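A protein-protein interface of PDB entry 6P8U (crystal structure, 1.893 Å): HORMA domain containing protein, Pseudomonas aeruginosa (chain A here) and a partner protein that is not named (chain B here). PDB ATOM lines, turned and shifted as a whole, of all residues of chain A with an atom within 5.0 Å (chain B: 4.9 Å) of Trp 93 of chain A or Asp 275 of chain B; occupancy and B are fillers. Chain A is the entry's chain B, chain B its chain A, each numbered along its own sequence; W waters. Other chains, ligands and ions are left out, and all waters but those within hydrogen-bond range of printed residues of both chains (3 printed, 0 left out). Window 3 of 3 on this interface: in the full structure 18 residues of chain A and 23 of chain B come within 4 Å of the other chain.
Water W2 lies within hydrogen-bond range of the backbone carbonyl oxygen of Ser 271 of chain B (2.9 Å), the guanidinium group of Arg 278 of chain B (3.0 Å) and the side-chain carboxylate of Asp 95 of chain A (3.4 Å). Water W1 lies within hydrogen-bond range of OG of Ser 271 of chain B, N of Ser 149 of chain A and OE1 of Gln 268 of chain B. Water W3 bridges the side-chain amide oxygen of Gln 268 of chain B and the side-chain carboxylate of Glu 152 of chain A.
Among the printed residues, merely in contact across the chains: Trp 93 of chain A with Gln 268 of chain B, Trp 93 of chain A with Ser 271 of chain B, Trp 93 of chain A with Asp 275 of chain B, Trp 93 of chain A with Arg 278 of chain B, Asp 95 of chain A with Ile 274 of chain B, Ser 149 of chain A with Gln 268 of chain B and Ser 149 of chain A with Ser 271 of chain B.
The backbone carbonyl oxygen (O) of Thr 150 of chain A is in hydrogen-bond range of the backbone NH (N) of Asp 95 of chain A. The guanidinium group (NH2) of Arg 281 of chain B lies within salt-bridge range of the side-chain carboxylate (OD2) of Asp 275 of chain B (3.9 Å). NH2 of Arg 278 of chain B is in salt-bridge range of OD1 of Asp 275 of chain B (2.8 Å). The side-chain carboxylate of Asp 275 of chain B is in salt-bridge range of the guanidinium group of Arg 279 of chain B, 3.5 Å away. The side-chain hydroxyl of Ser 149 of chain A lies within hydrogen-bond range of the side-chain carboxylate of Glu 152 of chain A (2.6 Å). NE1 of Trp 93 of chain A sits at hydrogen-bond distance from O of Ser 149 of chain A, at 3.4 Å.
Hydrophobic or aromatic side chains of chain A within 4 Å of the printed part of chain B: Trp 93. Of the 11 printed residues of chain B, 5 touch a printed residue of chain A. Hydrophobic or aromatic side chains of chain B that line the printed part of chain A: Ile 274.
Of chain B, only Gln 268 (3.9 Å), Ser 271 (3.8 Å), Asp 275 (3.3 Å) and Arg 278 (3.3 Å) come within 4 Å of Trp 93 of chain A. Of chain A, only Trp 93 (3.3 Å) comes within 4 Å of Asp 275 of chain B. Printed residues of chain B within 4 Å of Glu 152 of chain A: Gln 268 (3.0 Å). Printed residues of chain A within 4 Å of Ser 271 of chain B: Trp 93 (3.8 Å) and Ser 149 (3.7 Å). The nearest residue of chain B that does not touch Trp 93 of chain A is Ile 272 of chain B (4.1 Å). The nearest residue of chain A that does not touch Asp 275 of chain B is Phe 92 of chain A (4.2 Å).
OD2 of Asp 95 of chain A is in salt-bridge range of NH1 of Arg 278 of chain B. The side-chain carboxylate (OE1) of Glu 152 of chain A lies within hydrogen-bond range of the side-chain amide nitrogen (NE2) of Gln 268 of chain B, 3.0 Å away.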
ATOM      1  N   TYR A  15      25.497   8.150  -9.214  1.00  0.00           N
ATOM      2  CA  TYR A  15      24.259   8.919  -9.217  1.00  0.00           C
ATOM      3  C   TYR A  15      23.388   8.553 -10.413  1.00  0.00           C
ATOM      4  O   TYR A  15      22.193   8.275 -10.268  1.00  0.00           O
ATOM      5  CB  TYR A  15      24.555  10.407  -9.240  1.00  0.00           C
ATOM      6  CG  TYR A  15      23.311  11.261  -9.209  1.00  0.00           C
ATOM      7  CD1 TYR A  15      22.746  11.656  -8.003  1.00  0.00           C
ATOM      8  CD2 TYR A  15      22.702  11.668 -10.379  1.00  0.00           C
ATOM      9  CE1 TYR A  15      21.611  12.439  -7.964  1.00  0.00           C
ATOM     10  CE2 TYR A  15      21.557  12.466 -10.356  1.00  0.00           C
ATOM     11  CZ  TYR A  15      21.024  12.842  -9.138  1.00  0.00           C
ATOM     12  OH  TYR A  15      19.888  13.604  -9.097  1.00  0.00           O
ATOM     13  N   SER A  91      25.925  20.716 -12.155  1.00  0.00           N
ATOM     14  CA  SER A  91      24.585  20.530 -11.627  1.00  0.00           C
ATOM     15  C   SER A  91      24.064  19.126 -11.946  1.00  0.00           C
ATOM     16  O   SER A  91      24.513  18.445 -12.883  1.00  0.00           O
ATOM     17  CB  SER A  91      23.639  21.602 -12.170  1.00  0.00           C
ATOM     18  OG  SER A  91      23.984  21.977 -13.483  1.00  0.00           O
ATOM     19  N   PHE A  92      23.112  18.687 -11.129  1.00  0.00           N
ATOM     20  CA  PHE A  92      22.544  17.355 -11.238  1.00  0.00           C
ATOM     21  C   PHE A  92      21.060  17.422 -10.918  1.00  0.00           C
ATOM     22  O   PHE A  92      20.586  18.381 -10.304  1.00  0.00           O
ATOM     23  CB  PHE A  92      23.250  16.369 -10.297  1.00  0.00           C
ATOM     24  CG  PHE A  92      23.221  16.780  -8.857  1.00  0.00           C
ATOM     25  CD1 PHE A  92      24.159  17.661  -8.356  1.00  0.00           C
ATOM     26  CD2 PHE A  92      22.265  16.274  -8.002  1.00  0.00           C
ATOM     27  CE1 PHE A  92      24.135  18.036  -7.022  1.00  0.00           C
ATOM     28  CE2 PHE A  92      22.232  16.646  -6.670  1.00  0.00           C
ATOM     29  CZ  PHE A  92      23.165  17.526  -6.179  1.00  0.00           C
ATOM     30  N   TRP A  93      20.331  16.385 -11.336  1.00  0.00           N
ATOM     31  CA  TRP A  93      18.902  16.310 -11.084  1.00  0.00           C
ATOM     32  C   TRP A  93      18.383  14.957 -11.548  1.00  0.00           C
ATOM     33  O   TRP A  93      19.012  14.277 -12.369  1.00  0.00           O
ATOM     34  CB  TRP A  93      18.151  17.447 -11.795  1.00  0.00           C
ATOM     35  CG  TRP A  93      18.368  17.485 -13.286  1.00  0.00           C
ATOM     36  CD1 TRP A  93      17.922  16.582 -14.206  1.00  0.00           C
ATOM     37  CD2 TRP A  93      19.069  18.490 -14.020  1.00  0.00           C
ATOM     38  NE1 TRP A  93      18.315  16.958 -15.472  1.00  0.00           N
ATOM     39  CE2 TRP A  93      19.017  18.129 -15.385  1.00  0.00           C
ATOM     40  CE3 TRP A  93      19.726  19.669 -13.661  1.00  0.00           C
ATOM     41  CZ2 TRP A  93      19.614  18.899 -16.389  1.00  0.00           C
ATOM     42  CZ3 TRP A  93      20.319  20.439 -14.662  1.00  0.00           C
ATOM     43  CH2 TRP A  93      20.256  20.052 -16.005  1.00  0.00           C
ATOM     44  N   THR A  94      17.237  14.568 -10.988  1.00  0.00           N
ATOM     45  CA  THR A  94      16.457  13.420 -11.450  1.00  0.00           C
ATOM     46  C   THR A  94      15.040  13.947 -11.659  1.00  0.00           C
ATOM     47  O   THR A  94      14.305  14.168 -10.687  1.00  0.00           O
ATOM     48  CB  THR A  94      16.485  12.277 -10.449  1.00  0.00           C
ATOM     49  OG1 THR A  94      17.848  11.905 -10.188  1.00  0.00           O
ATOM     50  CG2 THR A  94      15.744  11.069 -11.004  1.00  0.00           C
ATOM     51  N   ASP A  95      14.669  14.169 -12.924  1.00  0.00           N
ATOM     52  CA  ASP A  95      13.463  14.936 -13.261  1.00  0.00           C
ATOM     53  C   ASP A  95      12.284  13.978 -13.418  1.00  0.00           C
ATOM     54  O   ASP A  95      11.874  13.603 -14.522  1.00  0.00           O
ATOM     55  CB  ASP A  95      13.702  15.754 -14.530  1.00  0.00           C
ATOM     56  CG  ASP A  95      12.708  16.875 -14.699  1.00  0.00           C
ATOM     57  OD1 ASP A  95      11.683  16.879 -13.964  1.00  0.00           O
ATOM     58  OD2 ASP A  95      12.946  17.769 -15.555  1.00  0.00           O
ATOM     59  N   SER A 149      17.128  15.795 -21.021  1.00  0.00           N
ATOM     60  CA  SER A 149      17.943  15.223 -19.956  1.00  0.00           C
ATOM     61  C   SER A 149      17.050  14.848 -18.780  1.00  0.00           C
ATOM     62  O   SER A 149      16.511  15.720 -18.092  1.00  0.00           O
ATOM     63  CB  SER A 149      19.019  16.215 -19.530  1.00  0.00           C
ATOM     64  OG  SER A 149      19.747  15.707 -18.433  1.00  0.00           O
ATOM     65  N   THR A 150      16.899  13.549 -18.542  1.00  0.00           N
ATOM     66  CA  THR A 150      16.070  13.055 -17.452  1.00  0.00           C
ATOM     67  C   THR A 150      16.865  12.917 -16.158  1.00  0.00           C
ATOM     68  O   THR A 150      16.415  13.357 -15.094  1.00  0.00           O
ATOM     69  CB  THR A 150      15.451  11.704 -17.831  1.00  0.00           C
ATOM     70  OG1 THR A 150      14.804  11.808 -19.111  1.00  0.00           O
ATOM     71  CG2 THR A 150      14.434  11.280 -16.785  1.00  0.00           C
ATOM     72  N   VAL A 151      18.037  12.296 -16.236  1.00  0.00           N
ATOM     73  CA  VAL A 151      18.922  12.093 -15.097  1.00  0.00           C
ATOM     74  C   VAL A 151      20.261  12.702 -15.477  1.00  0.00           C
ATOM     75  O   VAL A 151      20.851  12.331 -16.502  1.00  0.00           O
ATOM     76  CB  VAL A 151      19.067  10.608 -14.733  1.00  0.00           C
ATOM     77  CG1 VAL A 151      20.025  10.452 -13.546  1.00  0.00           C
ATOM     78  CG2 VAL A 151      17.715  10.009 -14.408  1.00  0.00           C
ATOM     79  N   GLU A 152      20.742  13.624 -14.650  1.00  0.00           N
ATOM     80  CA  GLU A 152      21.913  14.426 -14.970  1.00  0.00           C
ATOM     81  C   GLU A 152      22.841  14.501 -13.767  1.00  0.00           C
ATOM     82  O   GLU A 152      22.391  14.687 -12.630  1.00  0.00           O
ATOM     83  CB  GLU A 152      21.489  15.860 -15.397  1.00  0.00           C
ATOM     84  CG  GLU A 152      22.631  16.804 -15.730  1.00  0.00           C
ATOM     85  CD  GLU A 152      23.019  16.758 -17.193  1.00  0.00           C
ATOM     86  OE1 GLU A 152      22.130  16.636 -18.058  1.00  0.00           O
ATOM     87  OE2 GLU A 152      24.221  16.846 -17.490  1.00  0.00           O
ATOM     88  N   GLN B 268      19.480  21.015 -23.814  1.00  0.00           N
ATOM     89  CA  GLN B 268      20.171  21.059 -22.530  1.00  0.00           C
ATOM     90  C   GLN B 268      19.944  22.392 -21.827  1.00  0.00           C
ATOM     91  O   GLN B 268      19.744  22.423 -20.605  1.00  0.00           O
ATOM     92  CB  GLN B 268      21.663  20.800 -22.741  1.00  0.00           C
ATOM     93  CG  GLN B 268      22.450  20.561 -21.453  1.00  0.00           C
ATOM     94  CD  GLN B 268      21.936  19.361 -20.666  1.00  0.00           C
ATOM     95  OE1 GLN B 268      21.298  18.451 -21.219  1.00  0.00           O
ATOM     96  NE2 GLN B 268      22.205  19.359 -19.366  1.00  0.00           N
ATOM     97  N   SER B 271      16.612  22.276 -20.258  1.00  0.00           N
ATOM     98  CA  SER B 271      16.663  21.478 -19.040  1.00  0.00           C
ATOM     99  C   SER B 271      17.248  22.284 -17.892  1.00  0.00           C
ATOM    100  O   SER B 271      16.747  22.222 -16.768  1.00  0.00           O
ATOM    101  CB  SER B 271      17.481  20.206 -19.274  1.00  0.00           C
ATOM    102  OG  SER B 271      16.939  19.438 -20.338  1.00  0.00           O
ATOM    103  N   ILE B 272      18.319  23.038 -18.158  1.00  0.00           N
ATOM    104  CA  ILE B 272      18.918  23.891 -17.134  1.00  0.00           C
ATOM    105  C   ILE B 272      17.906  24.920 -16.647  1.00  0.00           C
ATOM    106  O   ILE B 272      17.822  25.206 -15.445  1.00  0.00           O
ATOM    107  CB  ILE B 272      20.199  24.562 -17.684  1.00  0.00           C
ATOM    108  CG1 ILE B 272      21.306  23.528 -17.844  1.00  0.00           C
ATOM    109  CG2 ILE B 272      20.646  25.703 -16.790  1.00  0.00           C
ATOM    110  CD1 ILE B 272      22.452  23.948 -18.743  1.00  0.00           C
ATOM    111  N   ALA B 273      17.133  25.504 -17.568  1.00  0.00           N
ATOM    112  CA  ALA B 273      16.150  26.508 -17.172  1.00  0.00           C
ATOM    113  C   ALA B 273      15.035  25.886 -16.336  1.00  0.00           C
ATOM    114  O   ALA B 273      14.546  26.503 -15.383  1.00  0.00           O
ATOM    115  CB  ALA B 273      15.572  27.194 -18.414  1.00  0.00           C
ATOM    116  N   ILE B 274      14.611  24.674 -16.692  1.00  0.00           N
ATOM    117  CA  ILE B 274      13.628  23.948 -15.899  1.00  0.00           C
ATOM    118  C   ILE B 274      14.189  23.632 -14.521  1.00  0.00           C
ATOM    119  O   ILE B 274      13.491  23.751 -13.507  1.00  0.00           O
ATOM    120  CB  ILE B 274      13.198  22.674 -16.655  1.00  0.00           C
ATOM    121  CG1 ILE B 274      12.344  23.077 -17.858  1.00  0.00           C
ATOM    122  CG2 ILE B 274      12.438  21.718 -15.733  1.00  0.00           C
ATOM    123  CD1 ILE B 274      12.203  21.971 -18.920  1.00  0.00           C
ATOM    124  N   ASP B 275      15.465  23.239 -14.455  1.00  0.00           N
ATOM    125  CA  ASP B 275      16.085  22.975 -13.159  1.00  0.00           C
ATOM    126  C   ASP B 275      16.107  24.232 -12.293  1.00  0.00           C
ATOM    127  O   ASP B 275      15.831  24.172 -11.086  1.00  0.00           O
ATOM    128  CB  ASP B 275      17.502  22.444 -13.361  1.00  0.00           C
ATOM    129  CG  ASP B 275      18.195  22.103 -12.055  1.00  0.00           C
ATOM    130  OD1 ASP B 275      17.701  21.217 -11.317  1.00  0.00           O
ATOM    131  OD2 ASP B 275      19.237  22.718 -11.769  1.00  0.00           O
ATOM    132  N   HIS B 276      16.439  25.384 -12.887  1.00  0.00           N
ATOM    133  CA  HIS B 276      16.420  26.636 -12.129  1.00  0.00           C
ATOM    134  C   HIS B 276      15.063  26.849 -11.462  1.00  0.00           C
ATOM    135  O   HIS B 276      14.977  27.123 -10.261  1.00  0.00           O
ATOM    136  CB  HIS B 276      16.731  27.818 -13.049  1.00  0.00           C
ATOM    137  CG  HIS B 276      18.183  28.009 -13.332  1.00  0.00           C
ATOM    138  ND1 HIS B 276      19.142  27.980 -12.346  1.00  0.00           N
ATOM    139  CD2 HIS B 276      18.841  28.269 -14.488  1.00  0.00           C
ATOM    140  CE1 HIS B 276      20.332  28.203 -12.878  1.00  0.00           C
ATOM    141  NE2 HIS B 276      20.179  28.374 -14.178  1.00  0.00           N
ATOM    142  N   ALA B 277      13.982  26.725 -12.236  1.00  0.00           N
ATOM    143  CA  ALA B 277      12.647  26.926 -11.683  1.00  0.00           C
ATOM    144  C   ALA B 277      12.326  25.886 -10.619  1.00  0.00           C
ATOM    145  O   ALA B 277      11.701  26.204  -9.601  1.00  0.00           O
ATOM    146  CB  ALA B 277      11.599  26.882 -12.799  1.00  0.00           C
ATOM    147  N   ARG B 278      12.739  24.634 -10.840  1.00  0.00           N
ATOM    148  CA  ARG B 278      12.519  23.588  -9.844  1.00  0.00           C
ATOM    149  C   ARG B 278      13.216  23.912  -8.524  1.00  0.00           C
ATOM    150  O   ARG B 278      12.699  23.589  -7.450  1.00  0.00           O
ATOM    151  CB  ARG B 278      13.004  22.252 -10.405  1.00  0.00           C
ATOM    152  CG  ARG B 278      12.759  21.051  -9.511  1.00  0.00           C
ATOM    153  CD  ARG B 278      13.019  19.735 -10.255  1.00  0.00           C
ATOM    154  NE  ARG B 278      14.342  19.687 -10.868  1.00  0.00           N
ATOM    155  CZ  ARG B 278      14.573  19.640 -12.182  1.00  0.00           C
ATOM    156  NH1 ARG B 278      13.563  19.641 -13.047  1.00  0.00           N
ATOM    157  NH2 ARG B 278      15.826  19.596 -12.633  1.00  0.00           N
ATOM    158  N   ARG B 279      14.370  24.566  -8.577  1.00  0.00           N
ATOM    159  CA  ARG B 279      15.094  24.969  -7.378  1.00  0.00           C
ATOM    160  C   ARG B 279      14.675  26.344  -6.870  1.00  0.00           C
ATOM    161  O   ARG B 279      15.350  26.908  -6.001  1.00  0.00           O
ATOM    162  CB  ARG B 279      16.593  24.965  -7.657  1.00  0.00           C
ATOM    163  CG  ARG B 279      17.126  23.637  -8.119  1.00  0.00           C
ATOM    164  CD  ARG B 279      18.586  23.722  -8.531  1.00  0.00           C
ATOM    165  NE  ARG B 279      19.269  22.460  -8.249  1.00  0.00           N
ATOM    166  CZ  ARG B 279      19.932  22.205  -7.124  1.00  0.00           C
ATOM    167  NH1 ARG B 279      20.019  23.129  -6.176  1.00  0.00           N
ATOM    168  NH2 ARG B 279      20.506  21.026  -6.953  1.00  0.00           N
ATOM    169  N   ARG B 281      14.734  29.206  -8.424  1.00  0.00           N
ATOM    170  CA  ARG B 281      15.510  30.309  -8.989  1.00  0.00           C
ATOM    171  C   ARG B 281      14.786  30.844 -10.223  1.00  0.00           C
ATOM    172  O   ARG B 281      15.174  30.623 -11.376  1.00  0.00           O
ATOM    173  CB  ARG B 281      16.923  29.841  -9.309  1.00  0.00           C
ATOM    174  CG  ARG B 281      17.612  29.151  -8.125  1.00  0.00           C
ATOM    175  CD  ARG B 281      19.108  28.974  -8.348  1.00  0.00           C
ATOM    176  NE  ARG B 281      19.406  27.912  -9.302  1.00  0.00           N
ATOM    177  CZ  ARG B 281      20.208  26.881  -9.063  1.00  0.00           C
ATOM    178  NH1 ARG B 281      20.828  26.769  -7.897  1.00  0.00           N
ATOM    179  NH2 ARG B 281      20.404  25.977 -10.010  1.00  0.00           N
HETATM  180  O   HOH W   1      18.329  18.048 -22.430  1.00  0.00           O
HETATM  181  O   HOH W   2      15.626  19.883 -15.585  1.00  0.00           O
HETATM  182  O   HOH W   3      22.543  15.846 -20.849  1.00  0.00           O
